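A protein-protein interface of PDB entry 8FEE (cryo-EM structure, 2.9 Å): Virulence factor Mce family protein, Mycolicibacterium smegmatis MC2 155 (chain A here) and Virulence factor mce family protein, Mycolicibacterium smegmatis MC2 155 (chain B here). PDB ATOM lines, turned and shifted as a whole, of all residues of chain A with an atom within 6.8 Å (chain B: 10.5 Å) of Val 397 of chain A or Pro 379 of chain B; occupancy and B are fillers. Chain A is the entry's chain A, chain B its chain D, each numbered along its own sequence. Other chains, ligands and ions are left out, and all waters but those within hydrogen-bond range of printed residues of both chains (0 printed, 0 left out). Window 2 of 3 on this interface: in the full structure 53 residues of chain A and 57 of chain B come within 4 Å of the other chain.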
ATOM      1  N   ALA A 394      35.196   6.605 -23.808  1.00  0.00           N
ATOM      2  CA  ALA A 394      33.970   5.956 -23.368  1.00  0.00           C
ATOM      3  C   ALA A 394      32.917   7.020 -23.102  1.00  0.00           C
ATOM      4  O   ALA A 394      33.223   8.210 -22.996  1.00  0.00           O
ATOM      5  CB  ALA A 394      34.199   5.102 -22.117  1.00  0.00           C
ATOM      6  N   GLU A 395      31.669   6.571 -23.005  1.00  0.00           N
ATOM      7  CA  GLU A 395      30.549   7.429 -22.654  1.00  0.00           C
ATOM      8  C   GLU A 395      29.714   6.731 -21.591  1.00  0.00           C
ATOM      9  O   GLU A 395      29.564   5.505 -21.615  1.00  0.00           O
ATOM     10  CB  GLU A 395      29.698   7.757 -23.889  1.00  0.00           C
ATOM     11  CG  GLU A 395      28.416   8.514 -23.601  1.00  0.00           C
ATOM     12  CD  GLU A 395      27.860   9.196 -24.829  1.00  0.00           C
ATOM     13  OE1 GLU A 395      28.622   9.385 -25.800  1.00  0.00           O
ATOM     14  OE2 GLU A 395      26.662   9.547 -24.823  1.00  0.00           O
ATOM     15  N   TYR A 396      29.176   7.514 -20.657  1.00  0.00           N
ATOM     16  CA  TYR A 396      28.368   6.997 -19.562  1.00  0.00           C
ATOM     17  C   TYR A 396      26.916   7.453 -19.657  1.00  0.00           C
ATOM     18  O   TYR A 396      26.229   7.577 -18.640  1.00  0.00           O
ATOM     19  CB  TYR A 396      28.979   7.412 -18.226  1.00  0.00           C
ATOM     20  CG  TYR A 396      30.429   7.008 -18.102  1.00  0.00           C
ATOM     21  CD1 TYR A 396      30.852   5.743 -18.481  1.00  0.00           C
ATOM     22  CD2 TYR A 396      31.380   7.903 -17.635  1.00  0.00           C
ATOM     23  CE1 TYR A 396      32.175   5.375 -18.380  1.00  0.00           C
ATOM     24  CE2 TYR A 396      32.706   7.544 -17.532  1.00  0.00           C
ATOM     25  CZ  TYR A 396      33.098   6.279 -17.907  1.00  0.00           C
ATOM     26  OH  TYR A 396      34.421   5.918 -17.804  1.00  0.00           O
ATOM     27  N   VAL A 397      26.438   7.709 -20.874  1.00  0.00           N
ATOM     28  CA  VAL A 397      25.029   8.006 -21.099  1.00  0.00           C
ATOM     29  C   VAL A 397      24.363   6.783 -21.714  1.00  0.00           C
ATOM     30  O   VAL A 397      23.446   6.200 -21.124  1.00  0.00           O
ATOM     31  CB  VAL A 397      24.854   9.242 -21.998  1.00  0.00           C
ATOM     32  CG1 VAL A 397      23.407   9.710 -21.981  1.00  0.00           C
ATOM     33  CG2 VAL A 397      25.789  10.356 -21.555  1.00  0.00           C
ATOM     34  N   TRP A 398      24.817   6.385 -22.903  1.00  0.00           N
ATOM     35  CA  TRP A 398      24.324   5.184 -23.563  1.00  0.00           C
ATOM     36  C   TRP A 398      25.353   4.061 -23.579  1.00  0.00           C
ATOM     37  O   TRP A 398      25.120   3.030 -24.219  1.00  0.00           O
ATOM     38  CB  TRP A 398      23.872   5.504 -24.990  1.00  0.00           C
ATOM     39  CG  TRP A 398      22.715   6.455 -25.055  1.00  0.00           C
ATOM     40  CD1 TRP A 398      21.407   6.174 -24.789  1.00  0.00           C
ATOM     41  CD2 TRP A 398      22.761   7.840 -25.420  1.00  0.00           C
ATOM     42  NE1 TRP A 398      20.636   7.298 -24.959  1.00  0.00           N
ATOM     43  CE2 TRP A 398      21.443   8.334 -25.348  1.00  0.00           C
ATOM     44  CE3 TRP A 398      23.787   8.710 -25.800  1.00  0.00           C
ATOM     45  CZ2 TRP A 398      21.125   9.660 -25.640  1.00  0.00           C
ATOM     46  CZ3 TRP A 398      23.470  10.025 -26.089  1.00  0.00           C
ATOM     47  CH2 TRP A 398      22.150  10.487 -26.007  1.00  0.00           C
ATOM     48  N   GLY A 399      26.475   4.231 -22.887  1.00  0.00           N
ATOM     49  CA  GLY A 399      27.472   3.175 -22.781  1.00  0.00           C
ATOM     50  C   GLY A 399      28.100   2.758 -24.093  1.00  0.00           C
ATOM     51  O   GLY A 399      28.334   1.564 -24.311  1.00  0.00           O
ATOM     52  N   ARG A 400      28.382   3.714 -24.973  1.00  0.00           N
ATOM     53  CA  ARG A 400      28.990   3.431 -26.267  1.00  0.00           C
ATOM     54  C   ARG A 400      30.439   3.895 -26.251  1.00  0.00           C
ATOM     55  O   ARG A 400      30.711   5.084 -26.055  1.00  0.00           O
ATOM     56  CB  ARG A 400      28.216   4.126 -27.388  1.00  0.00           C
ATOM     57  CG  ARG A 400      28.742   3.842 -28.783  1.00  0.00           C
ATOM     58  CD  ARG A 400      27.631   3.972 -29.811  1.00  0.00           C
ATOM     59  NE  ARG A 400      26.908   5.229 -29.666  1.00  0.00           N
ATOM     60  CZ  ARG A 400      25.777   5.520 -30.296  1.00  0.00           C
ATOM     61  NH1 ARG A 400      25.205   4.661 -31.122  1.00  0.00           N
ATOM     62  NH2 ARG A 400      25.205   6.703 -30.088  1.00  0.00           N
ATOM     63  N   PHE B 375      25.195  15.738 -10.053  1.00  0.00           N
ATOM     64  CA  PHE B 375      25.501  14.521 -10.794  1.00  0.00           C
ATOM     65  C   PHE B 375      26.654  13.759 -10.149  1.00  0.00           C
ATOM     66  O   PHE B 375      27.494  14.347  -9.470  1.00  0.00           O
ATOM     67  CB  PHE B 375      25.824  14.851 -12.256  1.00  0.00           C
ATOM     68  CG  PHE B 375      26.959  15.825 -12.430  1.00  0.00           C
ATOM     69  CD1 PHE B 375      28.267  15.379 -12.532  1.00  0.00           C
ATOM     70  CD2 PHE B 375      26.713  17.185 -12.510  1.00  0.00           C
ATOM     71  CE1 PHE B 375      29.308  16.271 -12.696  1.00  0.00           C
ATOM     72  CE2 PHE B 375      27.750  18.083 -12.675  1.00  0.00           C
ATOM     73  CZ  PHE B 375      29.049  17.625 -12.769  1.00  0.00           C
ATOM     74  N   ASN B 376      26.685  12.441 -10.365  1.00  0.00           N
ATOM     75  CA  ASN B 376      27.708  11.611  -9.735  1.00  0.00           C
ATOM     76  C   ASN B 376      29.080  11.850 -10.355  1.00  0.00           C
ATOM     77  O   ASN B 376      30.074  12.009  -9.637  1.00  0.00           O
ATOM     78  CB  ASN B 376      27.319  10.136  -9.835  1.00  0.00           C
ATOM     79  CG  ASN B 376      26.091   9.802  -9.013  1.00  0.00           C
ATOM     80  OD1 ASN B 376      25.779  10.484  -8.038  1.00  0.00           O
ATOM     81  ND2 ASN B 376      25.387   8.746  -9.403  1.00  0.00           N
ATOM     82  N   TYR B 377      29.157  11.880 -11.682  1.00  0.00           N
ATOM     83  CA  TYR B 377      30.432  12.043 -12.370  1.00  0.00           C
ATOM     84  C   TYR B 377      30.166  12.562 -13.778  1.00  0.00           C
ATOM     85  O   TYR B 377      29.020  12.773 -14.181  1.00  0.00           O
ATOM     86  CB  TYR B 377      31.220  10.729 -12.403  1.00  0.00           C
ATOM     87  CG  TYR B 377      30.401   9.530 -12.830  1.00  0.00           C
ATOM     88  CD1 TYR B 377      30.234   9.220 -14.172  1.00  0.00           C
ATOM     89  CD2 TYR B 377      29.805   8.703 -11.890  1.00  0.00           C
ATOM     90  CE1 TYR B 377      29.485   8.127 -14.565  1.00  0.00           C
ATOM     91  CE2 TYR B 377      29.057   7.610 -12.274  1.00  0.00           C
ATOM     92  CZ  TYR B 377      28.902   7.325 -13.612  1.00  0.00           C
ATOM     93  OH  TYR B 377      28.159   6.233 -13.998  1.00  0.00           O
ATOM     94  N   LEU B 378      31.249  12.764 -14.527  1.00  0.00           N
ATOM     95  CA  LEU B 378      31.175  13.279 -15.887  1.00  0.00           C
ATOM     96  C   LEU B 378      30.720  12.180 -16.847  1.00  0.00           C
ATOM     97  O   LEU B 378      31.106  11.020 -16.689  1.00  0.00           O
ATOM     98  CB  LEU B 378      32.531  13.824 -16.328  1.00  0.00           C
ATOM     99  CG  LEU B 378      32.997  15.093 -15.617  1.00  0.00           C
ATOM    100  CD1 LEU B 378      34.417  15.448 -16.023  1.00  0.00           C
ATOM    101  CD2 LEU B 378      32.049  16.240 -15.918  1.00  0.00           C
ATOM    102  N   PRO B 379      29.895  12.519 -17.842  1.00  0.00           N
ATOM    103  CA  PRO B 379      29.421  11.497 -18.789  1.00  0.00           C
ATOM    104  C   PRO B 379      30.526  10.851 -19.607  1.00  0.00           C
ATOM    105  O   PRO B 379      30.333   9.734 -20.101  1.00  0.00           O
ATOM    106  CB  PRO B 379      28.453  12.275 -19.691  1.00  0.00           C
ATOM    107  CG  PRO B 379      28.050  13.460 -18.891  1.00  0.00           C
ATOM    108  CD  PRO B 379      29.242  13.820 -18.059  1.00  0.00           C
ATOM    109  N   PHE B 380      31.668  11.508 -19.771  1.00  0.00           N
ATOM    110  CA  PHE B 380      32.718  11.041 -20.659  1.00  0.00           C
ATOM    111  C   PHE B 380      33.969  10.684 -19.867  1.00  0.00           C
ATOM    112  O   PHE B 380      34.241  11.258 -18.810  1.00  0.00           O
ATOM    113  CB  PHE B 380      33.057  12.098 -21.720  1.00  0.00           C
ATOM    114  CG  PHE B 380      33.062  13.506 -21.193  1.00  0.00           C
ATOM    115  CD1 PHE B 380      34.190  14.027 -20.582  1.00  0.00           C
ATOM    116  CD2 PHE B 380      31.939  14.309 -21.314  1.00  0.00           C
ATOM    117  CE1 PHE B 380      34.197  15.321 -20.098  1.00  0.00           C
ATOM    118  CE2 PHE B 380      31.940  15.604 -20.832  1.00  0.00           C
ATOM    119  CZ  PHE B 380      33.070  16.110 -20.223  1.00  0.00           C
ATOM    120  N   GLY B 381      34.723   9.723 -20.396  1.00  0.00           N
ATOM    121  CA  GLY B 381      35.948   9.286 -19.764  1.00  0.00           C
ATOM    122  C   GLY B 381      37.012   9.029 -20.809  1.00  0.00           C
ATOM    123  O   GLY B 381      36.718   8.828 -21.989  1.00  0.00           O
ATOM    124  N   MET B 382      38.265   9.041 -20.359  1.00  0.00           N
ATOM    125  CA  MET B 382      39.387   8.877 -21.268  1.00  0.00           C
ATOM    126  C   MET B 382      40.478   8.052 -20.600  1.00  0.00           C
ATOM    127  O   MET B 382      40.587   7.999 -19.374  1.00  0.00           O
ATOM    128  CB  MET B 382      39.938  10.240 -21.716  1.00  0.00           C
ATOM    129  CG  MET B 382      40.761  10.200 -22.993  1.00  0.00           C
ATOM    130  SD  MET B 382      40.924  11.822 -23.762  1.00  0.00           S
ATOM    131  CE  MET B 382      41.269  11.357 -25.458  1.00  0.00           C
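Among the printed residues, merely in contact across the chains: Ala 394 of chain A with Phe 380 of chain B (3.7 Å), Glu 395 of chain A with Pro 379 of chain B (3.4 Å), Tyr 396 of chain A with Tyr 377 of chain B (3.6 Å), Tyr 396 of chain A with Leu 378 of chain B (3.3 Å) and Val 397 of chain A with Pro 379 of chain B (3.8 Å).
Printed residues of chain B within 4 Å of Ala 394 of chain A: Phe 380 and Gly 381.
Of chain B, only Pro 379 comes within 4 Å of Glu 395 of chain A.
Tyr 396 of chain A touches just these residues of chain B: Tyr 377 (3.6 Å), Leu 378 (3.3 Å) and Pro 379 (2.6 Å).
Of the printed residues of chain B, Val 397 of chain A touches Pro 379 (3.8 Å).
No residue of chain B comes within 4 Å of Trp 398 of chain A.
Of the printed residues of chain A, Leu 378 of chain B touches Tyr 396 (3.3 Å).
Printed residues of chain A within 4 Å of Gly 381 of chain B: Ala 394.
The nearest residue of chain A that does not touch Pro 379 of chain B is Ala 394 of chain A (4.4 Å).
The nearest printed residue of chain B that does not touch Ala 394 of chain A is Pro 379 of chain B (4.4 Å).
Of the 8 printed residues of chain B, 5 touch a printed residue of chain A.
Among the printed residues, 7 pairs touch across the chains.
Among the printed residues, no Asp or Glu carboxylate lies within 4 Å of a Lys or Arg side-chain nitrogen of the other chain.
The backbone NH of Tyr 396 of chain A lies within hydrogen-bond range of the backbone carbonyl oxygen of Pro 379 of chain B (2.6 Å).
O of Gly 381 of chain B sits at hydrogen-bond distance from N of Ala 394 of chain A.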
